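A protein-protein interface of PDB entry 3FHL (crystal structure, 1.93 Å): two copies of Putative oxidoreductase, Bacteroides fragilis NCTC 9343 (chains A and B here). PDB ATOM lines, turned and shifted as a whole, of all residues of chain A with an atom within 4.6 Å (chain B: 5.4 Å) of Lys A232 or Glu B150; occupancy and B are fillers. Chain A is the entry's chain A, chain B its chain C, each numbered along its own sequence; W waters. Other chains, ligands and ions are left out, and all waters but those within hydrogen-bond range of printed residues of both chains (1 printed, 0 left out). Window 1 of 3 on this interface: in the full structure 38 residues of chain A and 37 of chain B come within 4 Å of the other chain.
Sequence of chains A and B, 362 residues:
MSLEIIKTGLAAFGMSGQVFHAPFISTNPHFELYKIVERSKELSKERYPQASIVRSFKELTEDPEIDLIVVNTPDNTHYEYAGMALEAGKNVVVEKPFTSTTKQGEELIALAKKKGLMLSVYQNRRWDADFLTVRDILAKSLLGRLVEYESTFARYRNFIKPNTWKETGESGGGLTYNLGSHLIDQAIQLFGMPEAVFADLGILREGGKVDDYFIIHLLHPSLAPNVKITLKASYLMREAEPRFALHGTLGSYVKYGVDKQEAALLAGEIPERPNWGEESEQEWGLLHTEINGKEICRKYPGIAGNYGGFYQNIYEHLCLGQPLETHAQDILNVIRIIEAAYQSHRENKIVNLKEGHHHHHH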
ATOM      1  N   SER A 151     -13.178  -4.976  -6.163  1.00  0.00           N
ATOM      2  CA  SER A 151     -14.501  -4.734  -5.618  1.00  0.00           C
ATOM      3  C   SER A 151     -15.547  -4.997  -6.674  1.00  0.00           C
ATOM      4  O   SER A 151     -15.452  -4.513  -7.797  1.00  0.00           O
ATOM      5  CB  SER A 151     -14.629  -3.313  -5.046  1.00  0.00           C
ATOM      6  OG  SER A 151     -14.502  -2.358  -6.078  1.00  0.00           O
ATOM      7  N   THR A 152     -16.539  -5.806  -6.299  1.00  0.00           N
ATOM      8  CA  THR A 152     -17.562  -6.278  -7.230  1.00  0.00           C
ATOM      9  C   THR A 152     -18.971  -6.181  -6.653  1.00  0.00           C
ATOM     10  O   THR A 152     -19.216  -6.572  -5.516  1.00  0.00           O
ATOM     11  CB  THR A 152     -17.261  -7.749  -7.664  1.00  0.00           C
ATOM     12  OG1 THR A 152     -15.950  -7.807  -8.235  1.00  0.00           O
ATOM     13  CG2 THR A 152     -18.287  -8.295  -8.686  1.00  0.00           C
ATOM     14  N   PHE A 153     -19.888  -5.644  -7.446  1.00  0.00           N
ATOM     15  CA  PHE A 153     -21.309  -5.778  -7.166  1.00  0.00           C
ATOM     16  C   PHE A 153     -21.867  -6.959  -7.961  1.00  0.00           C
ATOM     17  O   PHE A 153     -22.064  -6.873  -9.184  1.00  0.00           O
ATOM     18  CB  PHE A 153     -22.059  -4.494  -7.526  1.00  0.00           C
ATOM     19  CG  PHE A 153     -22.017  -3.421  -6.455  1.00  0.00           C
ATOM     20  CD1 PHE A 153     -22.442  -3.684  -5.155  1.00  0.00           C
ATOM     21  CD2 PHE A 153     -21.627  -2.123  -6.775  1.00  0.00           C
ATOM     22  CE1 PHE A 153     -22.428  -2.677  -4.171  1.00  0.00           C
ATOM     23  CE2 PHE A 153     -21.613  -1.103  -5.805  1.00  0.00           C
ATOM     24  CZ  PHE A 153     -22.006  -1.388  -4.499  1.00  0.00           C
ATOM     25  N   LEU A 183     -18.546   2.191  -6.750  1.00  0.00           N
ATOM     26  CA  LEU A 183     -17.274   1.481  -6.791  1.00  0.00           C
ATOM     27  C   LEU A 183     -16.116   2.418  -7.090  1.00  0.00           C
ATOM     28  O   LEU A 183     -15.072   2.360  -6.444  1.00  0.00           O
ATOM     29  CB  LEU A 183     -17.318   0.341  -7.824  1.00  0.00           C
ATOM     30  CG  LEU A 183     -18.285  -0.800  -7.505  1.00  0.00           C
ATOM     31  CD1 LEU A 183     -18.006  -1.982  -8.421  1.00  0.00           C
ATOM     32  CD2 LEU A 183     -18.180  -1.256  -6.049  1.00  0.00           C
ATOM     33  N   TYR A 213     -23.068  -5.326 -17.461  1.00  0.00           N
ATOM     34  CA  TYR A 213     -21.784  -5.882 -17.058  1.00  0.00           C
ATOM     35  C   TYR A 213     -20.715  -4.810 -17.232  1.00  0.00           C
ATOM     36  O   TYR A 213     -20.698  -4.124 -18.245  1.00  0.00           O
ATOM     37  CB  TYR A 213     -21.410  -7.100 -17.941  1.00  0.00           C
ATOM     38  CG  TYR A 213     -20.019  -7.656 -17.653  1.00  0.00           C
ATOM     39  CD1 TYR A 213     -19.830  -8.658 -16.701  1.00  0.00           C
ATOM     40  CD2 TYR A 213     -18.899  -7.168 -18.322  1.00  0.00           C
ATOM     41  CE1 TYR A 213     -18.546  -9.148 -16.413  1.00  0.00           C
ATOM     42  CE2 TYR A 213     -17.621  -7.647 -18.046  1.00  0.00           C
ATOM     43  CZ  TYR A 213     -17.455  -8.652 -17.099  1.00  0.00           C
ATOM     44  OH  TYR A 213     -16.178  -9.121 -16.837  1.00  0.00           O
ATOM     45  N   PHE A 214     -19.793  -4.686 -16.276  1.00  0.00           N
ATOM     46  CA  PHE A 214     -18.562  -3.967 -16.570  1.00  0.00           C
ATOM     47  C   PHE A 214     -17.411  -4.557 -15.799  1.00  0.00           C
ATOM     48  O   PHE A 214     -17.604  -5.142 -14.738  1.00  0.00           O
ATOM     49  CB  PHE A 214     -18.683  -2.442 -16.287  1.00  0.00           C
ATOM     50  CG  PHE A 214     -18.901  -2.085 -14.809  1.00  0.00           C
ATOM     51  CD1 PHE A 214     -17.830  -2.048 -13.910  1.00  0.00           C
ATOM     52  CD2 PHE A 214     -20.167  -1.757 -14.342  1.00  0.00           C
ATOM     53  CE1 PHE A 214     -18.031  -1.722 -12.557  1.00  0.00           C
ATOM     54  CE2 PHE A 214     -20.381  -1.406 -12.998  1.00  0.00           C
ATOM     55  CZ  PHE A 214     -19.294  -1.389 -12.104  1.00  0.00           C
ATOM     56  N   ILE A 215     -16.221  -4.400 -16.351  1.00  0.00           N
ATOM     57  CA  ILE A 215     -14.998  -4.561 -15.605  1.00  0.00           C
ATOM     58  C   ILE A 215     -14.146  -3.326 -15.897  1.00  0.00           C
ATOM     59  O   ILE A 215     -14.026  -2.898 -17.042  1.00  0.00           O
ATOM     60  CB  ILE A 215     -14.262  -5.906 -15.934  1.00  0.00           C
ATOM     61  CG1 ILE A 215     -12.980  -6.032 -15.107  1.00  0.00           C
ATOM     62  CG2 ILE A 215     -13.957  -6.044 -17.449  1.00  0.00           C
ATOM     63  CD1 ILE A 215     -12.508  -7.471 -14.894  1.00  0.00           C
ATOM     64  N   THR A 230      -9.357  -3.578  -9.569  1.00  0.00           N
ATOM     65  CA  THR A 230     -10.396  -4.082 -10.438  1.00  0.00           C
ATOM     66  C   THR A 230     -11.742  -3.731  -9.855  1.00  0.00           C
ATOM     67  O   THR A 230     -12.041  -4.061  -8.700  1.00  0.00           O
ATOM     68  CB  THR A 230     -10.318  -5.632 -10.588  1.00  0.00           C
ATOM     69  OG1 THR A 230      -8.983  -6.016 -10.918  1.00  0.00           O
ATOM     70  CG2 THR A 230     -11.274  -6.115 -11.658  1.00  0.00           C
ATOM     71  N   LEU A 231     -12.576  -3.093 -10.668  1.00  0.00           N
ATOM     72  CA  LEU A 231     -13.945  -2.809 -10.278  1.00  0.00           C
ATOM     73  C   LEU A 231     -14.851  -3.557 -11.252  1.00  0.00           C
ATOM     74  O   LEU A 231     -14.623  -3.513 -12.460  1.00  0.00           O
ATOM     75  CB  LEU A 231     -14.236  -1.292 -10.357  1.00  0.00           C
ATOM     76  CG  LEU A 231     -13.170  -0.324  -9.831  1.00  0.00           C
ATOM     77  CD1 LEU A 231     -13.595   1.119 -10.063  1.00  0.00           C
ATOM     78  CD2 LEU A 231     -12.917  -0.550  -8.331  1.00  0.00           C
ATOM     79  N   LYS A 232     -15.863  -4.240 -10.724  1.00  0.00           N
ATOM     80  CA  LYS A 232     -16.767  -5.080 -11.520  1.00  0.00           C
ATOM     81  C   LYS A 232     -18.192  -5.019 -11.026  1.00  0.00           C
ATOM     82  O   LYS A 232     -18.435  -4.831  -9.846  1.00  0.00           O
ATOM     83  CB  LYS A 232     -16.366  -6.559 -11.441  1.00  0.00           C
ATOM     84  CG  LYS A 232     -15.250  -6.995 -12.332  1.00  0.00           C
ATOM     85  CD  LYS A 232     -15.002  -8.522 -12.192  1.00  0.00           C
ATOM     86  CE  LYS A 232     -15.962  -9.336 -13.034  1.00  0.00           C
ATOM     87  NZ  LYS A 232     -15.534 -10.773 -13.141  1.00  0.00           N
ATOM     88  N   ALA A 233     -19.138  -5.188 -11.943  1.00  0.00           N
ATOM     89  CA  ALA A 233     -20.516  -5.501 -11.589  1.00  0.00           C
ATOM     90  C   ALA A 233     -21.153  -6.278 -12.719  1.00  0.00           C
ATOM     91  O   ALA A 233     -20.753  -6.127 -13.873  1.00  0.00           O
ATOM     92  CB  ALA A 233     -21.345  -4.230 -11.258  1.00  0.00           C
ATOM     93  N   MET A 237     -24.434 -13.093 -12.166  1.00  0.00           N
ATOM     94  CA  MET A 237     -23.527 -13.788 -11.260  1.00  0.00           C
ATOM     95  C   MET A 237     -24.368 -14.546 -10.242  1.00  0.00           C
ATOM     96  O   MET A 237     -24.528 -14.095  -9.100  1.00  0.00           O
ATOM     97  CB  MET A 237     -22.569 -12.823 -10.542  1.00  0.00           C
ATOM     98  CG  MET A 237     -21.527 -12.147 -11.419  1.00  0.00           C
ATOM     99  SD  MET A 237     -20.305 -11.135 -10.512  1.00  0.00           S
ATOM    100  CE  MET A 237     -19.201 -10.734 -11.852  1.00  0.00           C
ATOM    101  N   GLU A 241     -19.302 -13.119  -6.831  1.00  0.00           N
ATOM    102  CA  GLU A 241     -17.897 -12.821  -6.585  1.00  0.00           C
ATOM    103  C   GLU A 241     -17.790 -11.907  -5.338  1.00  0.00           C
ATOM    104  O   GLU A 241     -18.796 -11.344  -4.909  1.00  0.00           O
ATOM    105  CB  GLU A 241     -17.268 -12.204  -7.834  1.00  0.00           C
ATOM    106  CG  GLU A 241     -17.004 -13.274  -8.873  1.00  0.00           C
ATOM    107  CD  GLU A 241     -16.717 -12.750 -10.252  1.00  0.00           C
ATOM    108  OE1 GLU A 241     -16.220 -11.617 -10.421  1.00  0.00           O
ATOM    109  OE2 GLU A 241     -16.978 -13.515 -11.189  1.00  0.00           O
ATOM    110  N   GLU B 148     -19.421 -15.413 -19.083  1.00  0.00           N
ATOM    111  CA  GLU B 148     -18.149 -15.015 -18.492  1.00  0.00           C
ATOM    112  C   GLU B 148     -17.310 -16.209 -18.063  1.00  0.00           C
ATOM    113  O   GLU B 148     -17.837 -17.172 -17.526  1.00  0.00           O
ATOM    114  CB  GLU B 148     -18.373 -14.068 -17.293  1.00  0.00           C
ATOM    115  CG  GLU B 148     -17.069 -13.611 -16.623  1.00  0.00           C
ATOM    116  CD  GLU B 148     -17.223 -12.404 -15.702  1.00  0.00           C
ATOM    117  OE1 GLU B 148     -18.283 -12.280 -15.042  1.00  0.00           O
ATOM    118  OE2 GLU B 148     -16.261 -11.597 -15.635  1.00  0.00           O
ATOM    119  N   TYR B 149     -16.003 -16.110 -18.296  1.00  0.00           N
ATOM    120  CA  TYR B 149     -15.050 -17.167 -17.996  1.00  0.00           C
ATOM    121  C   TYR B 149     -13.865 -16.514 -17.318  1.00  0.00           C
ATOM    122  O   TYR B 149     -13.198 -15.648 -17.903  1.00  0.00           O
ATOM    123  CB  TYR B 149     -14.595 -17.802 -19.321  1.00  0.00           C
ATOM    124  CG  TYR B 149     -13.473 -18.820 -19.257  1.00  0.00           C
ATOM    125  CD1 TYR B 149     -13.750 -20.173 -19.016  1.00  0.00           C
ATOM    126  CD2 TYR B 149     -12.148 -18.442 -19.488  1.00  0.00           C
ATOM    127  CE1 TYR B 149     -12.738 -21.114 -19.008  1.00  0.00           C
ATOM    128  CE2 TYR B 149     -11.119 -19.370 -19.472  1.00  0.00           C
ATOM    129  CZ  TYR B 149     -11.423 -20.711 -19.240  1.00  0.00           C
ATOM    130  OH  TYR B 149     -10.414 -21.631 -19.218  1.00  0.00           O
ATOM    131  N   GLU B 150     -13.609 -16.935 -16.088  1.00  0.00           N
ATOM    132  CA  GLU B 150     -12.462 -16.463 -15.322  1.00  0.00           C
ATOM    133  C   GLU B 150     -11.609 -17.637 -14.937  1.00  0.00           C
ATOM    134  O   GLU B 150     -12.116 -18.635 -14.415  1.00  0.00           O
ATOM    135  CB  GLU B 150     -12.917 -15.751 -14.053  1.00  0.00           C
ATOM    136  CG  GLU B 150     -13.740 -14.491 -14.337  1.00  0.00           C
ATOM    137  CD  GLU B 150     -14.568 -14.050 -13.152  1.00  0.00           C
ATOM    138  OE1 GLU B 150     -14.030 -13.938 -12.027  1.00  0.00           O
ATOM    139  OE2 GLU B 150     -15.768 -13.810 -13.352  1.00  0.00           O
ATOM    140  N   SER B 151     -10.313 -17.517 -15.168  1.00  0.00           N
ATOM    141  CA  SER B 151      -9.401 -18.610 -14.881  1.00  0.00           C
ATOM    142  C   SER B 151      -8.166 -18.013 -14.208  1.00  0.00           C
ATOM    143  O   SER B 151      -7.520 -17.129 -14.759  1.00  0.00           O
ATOM    144  CB  SER B 151      -9.062 -19.354 -16.196  1.00  0.00           C
ATOM    145  OG  SER B 151      -7.964 -20.241 -16.059  1.00  0.00           O
ATOM    146  N   THR B 152      -7.843 -18.496 -13.012  1.00  0.00           N
ATOM    147  CA  THR B 152      -6.800 -17.900 -12.196  1.00  0.00           C
ATOM    148  C   THR B 152      -5.923 -18.936 -11.514  1.00  0.00           C
ATOM    149  O   THR B 152      -6.448 -19.896 -10.960  1.00  0.00           O
ATOM    150  CB  THR B 152      -7.428 -17.039 -11.047  1.00  0.00           C
ATOM    151  OG1 THR B 152      -8.294 -16.054 -11.606  1.00  0.00           O
ATOM    152  CG2 THR B 152      -6.355 -16.362 -10.145  1.00  0.00           C
ATOM    153  N   LYS B 228     -16.974 -12.817 -21.834  1.00  0.00           N
ATOM    154  CA  LYS B 228     -15.959 -12.029 -21.169  1.00  0.00           C
ATOM    155  C   LYS B 228     -14.909 -12.948 -20.551  1.00  0.00           C
ATOM    156  O   LYS B 228     -15.253 -13.818 -19.753  1.00  0.00           O
ATOM    157  CB  LYS B 228     -16.627 -11.138 -20.111  1.00  0.00           C
ATOM    158  CG  LYS B 228     -17.736 -10.249 -20.678  1.00  0.00           C
ATOM    159  CD  LYS B 228     -17.164  -9.177 -21.617  1.00  0.00           C
ATOM    160  CE  LYS B 228     -18.235  -8.166 -22.017  1.00  0.00           C
ATOM    161  NZ  LYS B 228     -17.792  -7.341 -23.167  1.00  0.00           N
ATOM    162  N   THR B 230     -11.294 -13.452 -18.420  1.00  0.00           N
ATOM    163  CA  THR B 230     -10.225 -12.944 -17.555  1.00  0.00           C
ATOM    164  C   THR B 230      -9.282 -14.075 -17.192  1.00  0.00           C
ATOM    165  O   THR B 230      -9.713 -15.098 -16.650  1.00  0.00           O
ATOM    166  CB  THR B 230     -10.763 -12.344 -16.231  1.00  0.00           C
ATOM    167  OG1 THR B 230     -11.803 -11.415 -16.505  1.00  0.00           O
ATOM    168  CG2 THR B 230      -9.668 -11.616 -15.489  1.00  0.00           C
ATOM    169  N   ARG B 243      -9.988 -20.989  -8.926  1.00  0.00           N
ATOM    170  CA  ARG B 243      -9.289 -21.495 -10.093  1.00  0.00           C
ATOM    171  C   ARG B 243     -10.134 -21.211 -11.337  1.00  0.00           C
ATOM    172  O   ARG B 243      -9.621 -20.739 -12.345  1.00  0.00           O
ATOM    173  CB  ARG B 243      -9.020 -23.006  -9.938  1.00  0.00           C
ATOM    174  CG  ARG B 243      -8.446 -23.695 -11.192  1.00  0.00           C
ATOM    175  CD  ARG B 243      -6.972 -23.385 -11.444  1.00  0.00           C
ATOM    176  NE  ARG B 243      -6.566 -23.807 -12.786  1.00  0.00           N
ATOM    177  CZ  ARG B 243      -6.748 -23.084 -13.889  1.00  0.00           C
ATOM    178  NH1 ARG B 243      -6.348 -23.551 -15.065  1.00  0.00           N
ATOM    179  NH2 ARG B 243      -7.330 -21.896 -13.820  1.00  0.00           N
ATOM    180  N   PHE B 244     -11.430 -21.480 -11.236  1.00  0.00           N
ATOM    181  CA  PHE B 244     -12.374 -21.126 -12.290  1.00  0.00           C
ATOM    182  C   PHE B 244     -13.601 -20.477 -11.697  1.00  0.00           C
ATOM    183  O   PHE B 244     -14.100 -20.899 -10.648  1.00  0.00           O
ATOM    184  CB  PHE B 244     -12.824 -22.356 -13.087  1.00  0.00           C
ATOM    185  CG  PHE B 244     -11.789 -22.880 -14.057  1.00  0.00           C
ATOM    186  CD1 PHE B 244     -11.109 -24.068 -13.788  1.00  0.00           C
ATOM    187  CD2 PHE B 244     -11.496 -22.195 -15.240  1.00  0.00           C
ATOM    188  CE1 PHE B 244     -10.136 -24.563 -14.691  1.00  0.00           C
ATOM    189  CE2 PHE B 244     -10.535 -22.680 -16.129  1.00  0.00           C
ATOM    190  CZ  PHE B 244      -9.856 -23.860 -15.861  1.00  0.00           C
ATOM    191  N   ALA B 245     -14.100 -19.452 -12.378  1.00  0.00           N
ATOM    192  CA  ALA B 245     -15.437 -18.953 -12.091  1.00  0.00           C
ATOM    193  C   ALA B 245     -16.074 -18.714 -13.435  1.00  0.00           C
ATOM    194  O   ALA B 245     -15.578 -17.920 -14.220  1.00  0.00           O
ATOM    195  CB  ALA B 245     -15.395 -17.655 -11.274  1.00  0.00           C
ATOM    196  N   LEU B 246     -17.151 -19.438 -13.701  1.00  0.00           N
ATOM    197  CA  LEU B 246     -17.874 -19.287 -14.953  1.00  0.00           C
ATOM    198  C   LEU B 246     -19.275 -18.836 -14.633  1.00  0.00           C
ATOM    199  O   LEU B 246     -19.840 -19.270 -13.644  1.00  0.00           O
ATOM    200  CB  LEU B 246     -17.909 -20.616 -15.720  1.00  0.00           C
ATOM    201  CG  LEU B 246     -16.661 -20.964 -16.545  1.00  0.00           C
ATOM    202  CD1 LEU B 246     -15.520 -21.401 -15.678  1.00  0.00           C
ATOM    203  CD2 LEU B 246     -17.007 -22.081 -17.516  1.00  0.00           C
ATOM    204  N   HIS B 247     -19.829 -17.971 -15.477  1.00  0.00           N
ATOM    205  CA  HIS B 247     -21.165 -17.447 -15.243  1.00  0.00           C
ATOM    206  C   HIS B 247     -21.940 -17.570 -16.526  1.00  0.00           C
ATOM    207  O   HIS B 247     -21.428 -17.247 -17.588  1.00  0.00           O
ATOM    208  CB  HIS B 247     -21.108 -15.963 -14.785  1.00  0.00           C
ATOM    209  CG  HIS B 247     -20.416 -15.765 -13.465  1.00  0.00           C
ATOM    210  ND1 HIS B 247     -20.903 -16.284 -12.287  1.00  0.00           N
ATOM    211  CD2 HIS B 247     -19.264 -15.131 -13.147  1.00  0.00           C
ATOM    212  CE1 HIS B 247     -20.075 -15.990 -11.301  1.00  0.00           C
ATOM    213  NE2 HIS B 247     -19.074 -15.281 -11.794  1.00  0.00           N
HETATM  214  O   HOH W   1     -12.804 -10.935 -13.720  1.00  0.00           O
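3 positions are printed for both chains.
Of the 8 pairs that touch across the chains among the printed residues, none has its exchanged pair printed and touching as well.
Water W1 bridges the side-chain amino group of Lys A232 (2.8 Å) and the side-chain hydroxyl of Thr B230 (3.0 Å).
Of the 13 printed residues of chain A, 4 touch a printed residue of chain B.
Printed residues of chain A that touch a printed residue of chain B: Tyr A213, Lys A232, Met A237 and Glu A241.
Hydrophobic or aromatic side chains of chain A within 4 Å of the printed part of chain B: Tyr A213 and Met A237.
Among the printed residues, 8 pairs touch across the chains.
Among the printed residues, Asp or Glu carboxylates within 4 Å of a Lys or Arg side-chain nitrogen of the other chain: Lys A232 with Glu B148 (2.7 Å) and Lys A232 with Glu B150 (3.1 Å).
The side-chain hydroxyl (OH) of Tyr A213 sits at hydrogen-bond distance from the side-chain carboxylate (OE2) of Glu B148, at 2.8 Å.
The side-chain amino group (NZ) of Lys A232 lies within salt-bridge range of the side-chain carboxylate (OE2) of Glu B148 (2.7 Å).
The side-chain carboxylate (OE2) of Glu B150 lies within salt-bridge range of the side-chain amino group (NZ) of Lys A232 (3.1 Å).
OE2 of Glu A241 lies close to OE2 of Glu B150 (2.5 Å).
OE2 of Glu A241 sits at hydrogen-bond distance from NE2 of His B247.
Of chain B, only Glu B148 (2.7 Å) and Glu B150 (3.1 Å) come within 4 Å of Lys A232.
Of the printed residues of chain A, Glu B148 touches Tyr A213, Lys A232 and Met A237.
Printed residues of chain A within 4 Å of Lys B228: Tyr A213 (3.7 Å).
Printed residues of chain B within 4 Å of Glu A241: Glu B150 and His B247.
Of the printed residues of chain A, His B247 touches Met A237 (3.8 Å) and Glu A241 (2.8 Å).
Printed residues of chain B within 4 Å of Tyr A213: Glu B148 and Lys B228.
Thr B152 touches none of the printed residues of chain A.
Thr A230 touches none of the printed residues of chain B.
The nearest residue of chain B that does not touch Lys A232 is Thr B230 (5.1 Å).
Among the printed residues, merely in contact across the chains: Tyr A213 with Lys B228, Met A237 with Glu B148 and Met A237 with His B247.
The backbone carbonyl oxygen (O) of Ser A151 sits at hydrogen-bond distance from the backbone NH (N) of Lys A232 (3.0 Å).
The backbone NH (N) of Phe A153 sits at hydrogen-bond distance from the backbone carbonyl oxygen (O) of Lys A232, 2.9 Å away.
The side-chain amino group (NZ) of Lys A232 lies within salt-bridge range of the side-chain carboxylate (OE1) of Glu A241, at 2.9 Å.
The backbone NH of His B247 is in hydrogen-bond range of the backbone carbonyl oxygen of Glu B148 (3.0 Å).
The backbone NH (N) of Tyr B149 sits at hydrogen-bond distance from the backbone carbonyl oxygen (O) of Lys B228 (2.8 Å).
The backbone carbonyl oxygen (O) of Ala B245 sits at hydrogen-bond distance from the backbone NH (N) of Glu B150, at 2.9 Å.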
